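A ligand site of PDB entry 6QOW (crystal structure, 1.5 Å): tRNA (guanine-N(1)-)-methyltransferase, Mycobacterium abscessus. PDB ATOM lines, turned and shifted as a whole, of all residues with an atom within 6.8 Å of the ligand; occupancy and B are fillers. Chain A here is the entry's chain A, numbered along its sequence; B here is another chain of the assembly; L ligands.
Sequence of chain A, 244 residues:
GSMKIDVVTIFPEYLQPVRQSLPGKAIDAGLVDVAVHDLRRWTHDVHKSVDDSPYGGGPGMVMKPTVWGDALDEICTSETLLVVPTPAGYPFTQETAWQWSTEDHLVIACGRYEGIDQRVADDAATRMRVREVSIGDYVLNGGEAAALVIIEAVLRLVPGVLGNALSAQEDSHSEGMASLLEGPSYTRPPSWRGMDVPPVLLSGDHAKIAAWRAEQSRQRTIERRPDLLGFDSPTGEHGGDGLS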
ATOM      1  N   MET A  63      22.235  -8.850 -14.227  1.00  0.00           N
ATOM      2  CA  MET A  63      21.226  -8.635 -15.258  1.00  0.00           C
ATOM      3  C   MET A  63      21.464  -7.327 -16.022  1.00  0.00           C
ATOM      4  O   MET A  63      21.801  -6.278 -15.450  1.00  0.00           O
ATOM      5  CB  MET A  63      19.812  -8.679 -14.657  1.00  0.00           C
ATOM      6  CG  MET A  63      19.495 -10.023 -13.976  1.00  0.00           C
ATOM      7  SD  MET A  63      17.729 -10.269 -13.578  1.00  0.00           S
ATOM      8  CE  MET A  63      17.224 -11.431 -14.847  1.00  0.00           C
ATOM      9  N   VAL A  84      11.724  -3.169  -5.860  1.00  0.00           N
ATOM     10  CA  VAL A  84      12.834  -4.046  -6.292  1.00  0.00           C
ATOM     11  C   VAL A  84      13.312  -4.889  -5.103  1.00  0.00           C
ATOM     12  O   VAL A  84      14.069  -4.404  -4.233  1.00  0.00           O
ATOM     13  CB  VAL A  84      14.037  -3.235  -6.860  1.00  0.00           C
ATOM     14  CG1 VAL A  84      15.089  -4.173  -7.438  1.00  0.00           C
ATOM     15  CG2 VAL A  84      13.586  -2.240  -7.950  1.00  0.00           C
ATOM     16  N   PRO A  85      12.858  -6.152  -5.012  1.00  0.00           N
ATOM     17  CA  PRO A  85      13.349  -6.967  -3.894  1.00  0.00           C
ATOM     18  C   PRO A  85      14.848  -7.292  -4.005  1.00  0.00           C
ATOM     19  O   PRO A  85      15.330  -7.613  -5.096  1.00  0.00           O
ATOM     20  CB  PRO A  85      12.508  -8.246  -3.989  1.00  0.00           C
ATOM     21  CG  PRO A  85      11.236  -7.804  -4.713  1.00  0.00           C
ATOM     22  CD  PRO A  85      11.701  -6.753  -5.688  1.00  0.00           C
ATOM     23  N   THR A  86      15.566  -7.170  -2.888  1.00  0.00           N
ATOM     24  CA  THR A  86      17.011  -7.430  -2.869  1.00  0.00           C
ATOM     25  C   THR A  86      17.456  -7.678  -1.421  1.00  0.00           C
ATOM     26  O   THR A  86      16.911  -7.072  -0.507  1.00  0.00           O
ATOM     27  CB  THR A  86      17.825  -6.241  -3.488  1.00  0.00           C
ATOM     28  OG1 THR A  86      19.205  -6.370  -3.111  1.00  0.00           O
ATOM     29  CG2 THR A  86      17.298  -4.890  -3.039  1.00  0.00           C
ATOM     30  N   PRO A  87      18.449  -8.577  -1.211  1.00  0.00           N
ATOM     31  CA  PRO A  87      18.936  -8.785   0.162  1.00  0.00           C
ATOM     32  C   PRO A  87      19.518  -7.511   0.788  1.00  0.00           C
ATOM     33  O   PRO A  87      19.616  -7.448   2.026  1.00  0.00           O
ATOM     34  CB  PRO A  87      20.041  -9.836  -0.001  1.00  0.00           C
ATOM     35  CG  PRO A  87      19.856 -10.431  -1.331  1.00  0.00           C
ATOM     36  CD  PRO A  87      19.155  -9.419  -2.191  1.00  0.00           C
ATOM     37  N   ALA A  88      19.922  -6.550  -0.035  1.00  0.00           N
ATOM     38  CA  ALA A  88      20.494  -5.301   0.462  1.00  0.00           C
ATOM     39  C   ALA A  88      19.465  -4.184   0.632  1.00  0.00           C
ATOM     40  O   ALA A  88      19.830  -3.005   0.785  1.00  0.00           O
ATOM     41  CB  ALA A  88      21.608  -4.825  -0.471  1.00  0.00           C
ATOM     42  N   CYS A 110      11.701  -8.456 -10.532  1.00  0.00           N
ATOM     43  CA  CYS A 110      12.334  -9.626  -9.909  1.00  0.00           C
ATOM     44  C   CYS A 110      13.716  -9.946 -10.485  1.00  0.00           C
ATOM     45  O   CYS A 110      13.834 -10.302 -11.667  1.00  0.00           O
ATOM     46  CB  CYS A 110      11.452 -10.876 -10.062  1.00  0.00           C
ATOM     47  SG  CYS A 110       9.785 -10.756  -9.316  1.00  0.00           S
ATOM     48  N   GLY A 111      14.759  -9.835  -9.655  1.00  0.00           N
ATOM     49  CA  GLY A 111      16.092 -10.200 -10.093  1.00  0.00           C
ATOM     50  C   GLY A 111      16.421 -11.680  -9.957  1.00  0.00           C
ATOM     51  O   GLY A 111      15.743 -12.435  -9.236  1.00  0.00           O
ATOM     52  N   ARG A 112      17.450 -12.095 -10.691  1.00  0.00           N
ATOM     53  CA  ARG A 112      18.072 -13.423 -10.591  1.00  0.00           C
ATOM     54  C   ARG A 112      19.587 -13.188 -10.725  1.00  0.00           C
ATOM     55  O   ARG A 112      20.026 -12.043 -10.836  1.00  0.00           O
ATOM     56  CB  ARG A 112      17.538 -14.382 -11.665  1.00  0.00           C
ATOM     57  CG  ARG A 112      16.140 -14.976 -11.362  1.00  0.00           C
ATOM     58  CD  ARG A 112      16.247 -16.258 -10.525  1.00  0.00           C
ATOM     59  NE  ARG A 112      15.023 -16.548  -9.769  1.00  0.00           N
ATOM     60  CZ  ARG A 112      14.796 -17.695  -9.130  1.00  0.00           C
ATOM     61  NH1 ARG A 112      15.689 -18.688  -9.179  1.00  0.00           N
ATOM     62  NH2 ARG A 112      13.656 -17.859  -8.461  1.00  0.00           N
ATOM     63  N   TYR A 113      20.365 -14.276 -10.726  1.00  0.00           N
ATOM     64  CA  TYR A 113      21.831 -14.173 -10.687  1.00  0.00           C
ATOM     65  C   TYR A 113      22.260 -13.302  -9.492  1.00  0.00           C
ATOM     66  O   TYR A 113      21.702 -13.445  -8.397  1.00  0.00           O
ATOM     67  CB  TYR A 113      22.382 -13.631 -12.010  1.00  0.00           C
ATOM     68  CG  TYR A 113      21.874 -14.343 -13.247  1.00  0.00           C
ATOM     69  CD1 TYR A 113      20.701 -13.947 -13.888  1.00  0.00           C
ATOM     70  CD2 TYR A 113      22.560 -15.440 -13.763  1.00  0.00           C
ATOM     71  CE1 TYR A 113      20.238 -14.614 -15.001  1.00  0.00           C
ATOM     72  CE2 TYR A 113      22.101 -16.113 -14.888  1.00  0.00           C
ATOM     73  CZ  TYR A 113      20.941 -15.686 -15.505  1.00  0.00           C
ATOM     74  OH  TYR A 113      20.472 -16.347 -16.615  1.00  0.00           O
ATOM     75  N   GLU A 114      23.220 -12.403  -9.681  1.00  0.00           N
ATOM     76  CA  GLU A 114      23.681 -11.569  -8.565  1.00  0.00           C
ATOM     77  C   GLU A 114      22.845 -10.292  -8.364  1.00  0.00           C
ATOM     78  O   GLU A 114      23.064  -9.556  -7.400  1.00  0.00           O
ATOM     79  CB  GLU A 114      25.157 -11.205  -8.756  1.00  0.00           C
ATOM     80  CG  GLU A 114      26.081 -12.409  -8.773  1.00  0.00           C
ATOM     81  CD  GLU A 114      25.782 -13.399  -7.655  1.00  0.00           C
ATOM     82  OE1 GLU A 114      25.985 -13.036  -6.473  1.00  0.00           O
ATOM     83  OE2 GLU A 114      25.342 -14.531  -7.949  1.00  0.00           O
ATOM     84  N   GLY A 115      21.860 -10.051  -9.238  1.00  0.00           N
ATOM     85  CA  GLY A 115      21.031  -8.860  -9.151  1.00  0.00           C
ATOM     86  C   GLY A 115      21.012  -8.064 -10.456  1.00  0.00           C
ATOM     87  O   GLY A 115      21.543  -8.510 -11.480  1.00  0.00           O
ATOM     88  N   ILE A 116      20.410  -6.885 -10.394  1.00  0.00           N
ATOM     89  CA  ILE A 116      20.204  -6.012 -11.576  1.00  0.00           C
ATOM     90  C   ILE A 116      21.228  -4.864 -11.582  1.00  0.00           C
ATOM     91  O   ILE A 116      21.469  -4.268 -10.538  1.00  0.00           O
ATOM     92  CB  ILE A 116      18.769  -5.422 -11.591  1.00  0.00           C
ATOM     93  CG1 ILE A 116      17.712  -6.545 -11.479  1.00  0.00           C
ATOM     94  CG2 ILE A 116      18.541  -4.544 -12.831  1.00  0.00           C
ATOM     95  CD1 ILE A 116      16.274  -6.048 -11.314  1.00  0.00           C
ATOM     96  N   VAL A 133      13.821  -3.253  -1.292  1.00  0.00           N
ATOM     97  CA  VAL A 133      13.422  -3.859   0.003  1.00  0.00           C
ATOM     98  C   VAL A 133      13.802  -5.321   0.142  1.00  0.00           C
ATOM     99  O   VAL A 133      13.881  -6.043  -0.857  1.00  0.00           O
ATOM    100  CB  VAL A 133      11.873  -3.769   0.266  1.00  0.00           C
ATOM    101  CG1 VAL A 133      11.406  -2.307   0.346  1.00  0.00           C
ATOM    102  CG2 VAL A 133      11.063  -4.530  -0.797  1.00  0.00           C
ATOM    103  N   SER A 134      14.041  -5.751   1.379  1.00  0.00           N
ATOM    104  CA  SER A 134      14.242  -7.157   1.738  1.00  0.00           C
ATOM    105  C   SER A 134      13.084  -7.663   2.581  1.00  0.00           C
ATOM    106  O   SER A 134      12.563  -6.925   3.433  1.00  0.00           O
ATOM    107  CB  SER A 134      15.558  -7.334   2.496  1.00  0.00           C
ATOM    108  OG  SER A 134      15.603  -8.601   3.131  1.00  0.00           O
ATOM    109  N   ILE A 135      12.674  -8.914   2.370  1.00  0.00           N
ATOM    110  CA  ILE A 135      11.573  -9.485   3.186  1.00  0.00           C
ATOM    111  C   ILE A 135      12.095 -10.239   4.425  1.00  0.00           C
ATOM    112  O   ILE A 135      11.285 -10.728   5.233  1.00  0.00           O
ATOM    113  CB  ILE A 135      10.640 -10.426   2.355  1.00  0.00           C
ATOM    114  CG1 ILE A 135      11.382 -11.661   1.818  1.00  0.00           C
ATOM    115  CG2 ILE A 135       9.936  -9.630   1.229  1.00  0.00           C
ATOM    116  CD1 ILE A 135      10.441 -12.839   1.504  1.00  0.00           C
ATOM    117  N   GLY A 136      13.407 -10.332   4.605  1.00  0.00           N
ATOM    118  CA  GLY A 136      13.959 -10.974   5.809  1.00  0.00           C
ATOM    119  C   GLY A 136      15.440 -11.251   5.680  1.00  0.00           C
ATOM    120  O   GLY A 136      16.006 -11.144   4.587  1.00  0.00           O
ATOM    121  N   ASP A 137      16.089 -11.601   6.797  1.00  0.00           N
ATOM    122  CA  ASP A 137      17.554 -11.765   6.801  1.00  0.00           C
ATOM    123  C   ASP A 137      17.996 -13.183   6.431  1.00  0.00           C
ATOM    124  O   ASP A 137      18.542 -13.923   7.249  1.00  0.00           O
ATOM    125  CB  ASP A 137      18.120 -11.377   8.166  1.00  0.00           C
ATOM    126  CG  ASP A 137      18.052  -9.884   8.423  1.00  0.00           C
ATOM    127  OD1 ASP A 137      17.891  -9.127   7.447  1.00  0.00           O
ATOM    128  OD2 ASP A 137      18.172  -9.477   9.592  1.00  0.00           O
ATOM    129  N   TYR A 138      17.740 -13.520   5.172  1.00  0.00           N
ATOM    130  CA  TYR A 138      18.143 -14.772   4.554  1.00  0.00           C
ATOM    131  C   TYR A 138      18.336 -14.468   3.064  1.00  0.00           C
ATOM    132  O   TYR A 138      17.847 -13.435   2.577  1.00  0.00           O
ATOM    133  CB  TYR A 138      17.092 -15.883   4.751  1.00  0.00           C
ATOM    134  CG  TYR A 138      15.665 -15.376   4.717  1.00  0.00           C
ATOM    135  CD1 TYR A 138      15.045 -15.046   3.505  1.00  0.00           C
ATOM    136  CD2 TYR A 138      14.945 -15.177   5.889  1.00  0.00           C
ATOM    137  CE1 TYR A 138      13.748 -14.549   3.470  1.00  0.00           C
ATOM    138  CE2 TYR A 138      13.639 -14.683   5.877  1.00  0.00           C
ATOM    139  CZ  TYR A 138      13.053 -14.361   4.655  1.00  0.00           C
ATOM    140  OH  TYR A 138      11.768 -13.862   4.607  1.00  0.00           O
ATOM    141  N   VAL A 139      19.035 -15.351   2.370  1.00  0.00           N
ATOM    142  CA  VAL A 139      19.307 -15.145   0.947  1.00  0.00           C
ATOM    143  C   VAL A 139      18.484 -16.105   0.096  1.00  0.00           C
ATOM    144  O   VAL A 139      18.551 -17.312   0.267  1.00  0.00           O
ATOM    145  CB  VAL A 139      20.805 -15.329   0.634  1.00  0.00           C
ATOM    146  CG1 VAL A 139      21.074 -15.182  -0.854  1.00  0.00           C
ATOM    147  CG2 VAL A 139      21.631 -14.316   1.432  1.00  0.00           C
ATOM    148  N   LEU A 140      17.686 -15.552  -0.818  1.00  0.00           N
ATOM    149  CA  LEU A 140      16.970 -16.354  -1.817  1.00  0.00           C
ATOM    150  C   LEU A 140      17.785 -16.514  -3.118  1.00  0.00           C
ATOM    151  O   LEU A 140      18.855 -15.911  -3.270  1.00  0.00           O
ATOM    152  CB  LEU A 140      15.607 -15.706  -2.119  1.00  0.00           C
ATOM    153  CG  LEU A 140      14.702 -15.465  -0.905  1.00  0.00           C
ATOM    154  CD1 LEU A 140      13.495 -14.637  -1.300  1.00  0.00           C
ATOM    155  CD2 LEU A 140      14.261 -16.795  -0.287  1.00  0.00           C
ATOM    156  N   ASN A 141      17.280 -17.306  -4.059  1.00  0.00           N
ATOM    157  CA  ASN A 141      17.898 -17.371  -5.400  1.00  0.00           C
ATOM    158  C   ASN A 141      17.495 -16.199  -6.306  1.00  0.00           C
ATOM    159  O   ASN A 141      18.228 -15.853  -7.241  1.00  0.00           O
ATOM    160  CB  ASN A 141      17.514 -18.672  -6.109  1.00  0.00           C
ATOM    161  CG  ASN A 141      18.227 -19.887  -5.545  1.00  0.00           C
ATOM    162  OD1 ASN A 141      19.392 -19.809  -5.149  1.00  0.00           O
ATOM    163  ND2 ASN A 141      17.522 -21.012  -5.514  1.00  0.00           N
ATOM    164  N   GLY A 142      16.335 -15.616  -6.051  1.00  0.00           N
ATOM    165  CA  GLY A 142      15.860 -14.508  -6.860  1.00  0.00           C
ATOM    166  C   GLY A 142      14.686 -13.819  -6.182  1.00  0.00           C
ATOM    167  O   GLY A 142      14.284 -14.221  -5.073  1.00  0.00           O
ATOM    168  N   GLY A 143      14.143 -12.807  -6.838  1.00  0.00           N
ATOM    169  CA  GLY A 143      13.089 -11.986  -6.253  1.00  0.00           C
ATOM    170  C   GLY A 143      11.663 -12.532  -6.258  1.00  0.00           C
ATOM    171  O   GLY A 143      10.791 -11.937  -5.617  1.00  0.00           O
ATOM    172  N   GLU A 144      11.428 -13.653  -6.943  1.00  0.00           N
ATOM    173  CA  GLU A 144      10.054 -14.145  -7.137  1.00  0.00           C
ATOM    174  C   GLU A 144       9.328 -14.512  -5.832  1.00  0.00           C
ATOM    175  O   GLU A 144       8.168 -14.125  -5.649  1.00  0.00           O
ATOM    176  CB  GLU A 144      10.058 -15.346  -8.094  1.00  0.00           C
ATOM    177  CG  GLU A 144      10.336 -14.972  -9.567  1.00  0.00           C
ATOM    178  CD  GLU A 144      11.811 -14.745  -9.903  1.00  0.00           C
ATOM    179  OE1 GLU A 144      12.692 -15.036  -9.068  1.00  0.00           O
ATOM    180  OE2 GLU A 144      12.102 -14.281 -11.025  1.00  0.00           O
ATOM    181  N   ALA A 146       9.941 -13.324  -2.915  1.00  0.00           N
ATOM    182  CA  ALA A 146       9.720 -12.046  -2.238  1.00  0.00           C
ATOM    183  C   ALA A 146       8.492 -11.320  -2.807  1.00  0.00           C
ATOM    184  O   ALA A 146       7.698 -10.746  -2.051  1.00  0.00           O
ATOM    185  CB  ALA A 146      10.970 -11.149  -2.338  1.00  0.00           C
ATOM    186  N   GLU B 152      13.278 -22.504  -0.498  1.00  0.00           N
ATOM    187  CA  GLU B 152      14.289 -21.928  -1.386  1.00  0.00           C
ATOM    188  C   GLU B 152      15.557 -21.561  -0.617  1.00  0.00           C
ATOM    189  O   GLU B 152      16.672 -21.852  -1.094  1.00  0.00           O
ATOM    190  CB  GLU B 152      13.729 -20.693  -2.107  1.00  0.00           C
ATOM    191  CG  GLU B 152      14.717 -20.019  -3.042  1.00  0.00           C
ATOM    192  CD  GLU B 152      14.048 -19.000  -3.951  1.00  0.00           C
ATOM    193  OE1 GLU B 152      12.815 -19.116  -4.203  1.00  0.00           O
ATOM    194  OE2 GLU B 152      14.736 -18.083  -4.430  1.00  0.00           O
HETATM  195  C1  LIG L   1      15.734 -11.437  -0.945  1.00  0.00           C
HETATM  196  C2  LIG L   1      19.002 -11.868  -7.262  1.00  0.00           C
HETATM  197  O1  LIG L   1      17.720 -11.498  -6.761  1.00  0.00           O
HETATM  198  C3  LIG L   1      17.515 -11.705  -5.395  1.00  0.00           C
HETATM  199  C4  LIG L   1      18.302 -12.595  -4.675  1.00  0.00           C
HETATM  200  C5  LIG L   1      18.082 -12.786  -3.313  1.00  0.00           C
HETATM  201  C6  LIG L   1      17.045 -12.084  -2.674  1.00  0.00           C
HETATM  202  C7  LIG L   1      16.255 -11.206  -3.406  1.00  0.00           C
HETATM  203  C8  LIG L   1      16.482 -11.009  -4.769  1.00  0.00           C
HETATM  204  S1  LIG L   1      15.098 -10.546  -2.286  1.00  0.00           S
HETATM  205  N1  LIG L   1      16.757 -12.201  -1.332  1.00  0.00           N
HETATM  206  C9  LIG L   1      15.139 -11.247   0.417  1.00  0.00           C
HETATM  207  O2  LIG L   1      15.621 -11.820   1.442  1.00  0.00           O
HETATM  208  O3  LIG L   1      14.234 -10.388   0.493  1.00  0.00           O
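An oxygen (O3) of the ligand is in hydrogen-bond range of the backbone NH of Ile 135. O of Tyr 138 sits close to O2 of the ligand (3.0 Å). N of Thr 86 sits close to S1 of the ligand, 3.5 Å away. An oxygen (O3) of the ligand lies close to the side-chain hydroxyl of Ser 134.
O of Gly 111 lies close to O1 of the ligand, at 3.3 Å. The backbone carbonyl oxygen of Gly 136 sits close to an oxygen (O2) of the ligand, at 3.2 Å. Residues that only touch the ligand: Leu 140 (3.2 Å), Tyr 113 (3.3 Å), Pro 87 (3.4 Å), Gly 142 (3.5 Å), Pro 85 (3.6 Å), Gly 143 (3.6 Å), Arg 112 (3.7 Å) and Gly 115 (3.9 Å). Hydrophobic or aromatic side chains that line the ligand: Pro 85, Pro 87, Ile 135, Tyr 138 and Leu 140. Within 4 Å of the ligand: Pro 85, Thr 86, Pro 87, Gly 111, Arg 112, Tyr 113, Gly 115, Ser 134, Ile 135, Gly 136, Tyr 138, Leu 140, Gly 142 and Gly 143.
OH of Tyr 138 lies within hydrogen-bond range of O of Ile 135. The side-chain hydroxyl of Ser 134 is in hydrogen-bond range of the backbone carbonyl oxygen of Gly 136, 3.0 Å away. N of Gly 143 is in hydrogen-bond range of O of Gly 111. O of Val 133 is in hydrogen-bond range of N of Thr 86. The side-chain carboxylate of Glu 152 of chain B is in hydrogen-bond range of the backbone NH of Gly 142 (3.4 Å). NE of Arg 112 lies within salt-bridge range of OE1 of Glu 144, 2.9 Å away. The side-chain sulfur (SD) of Met 63 sits at hydrogen-bond distance from the backbone NH (N) of Arg 112, 3.4 Å away. The backbone carbonyl oxygen (O) of Gly 115 sits at hydrogen-bond distance from the backbone NH (N) of Met 63, 2.9 Å away.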
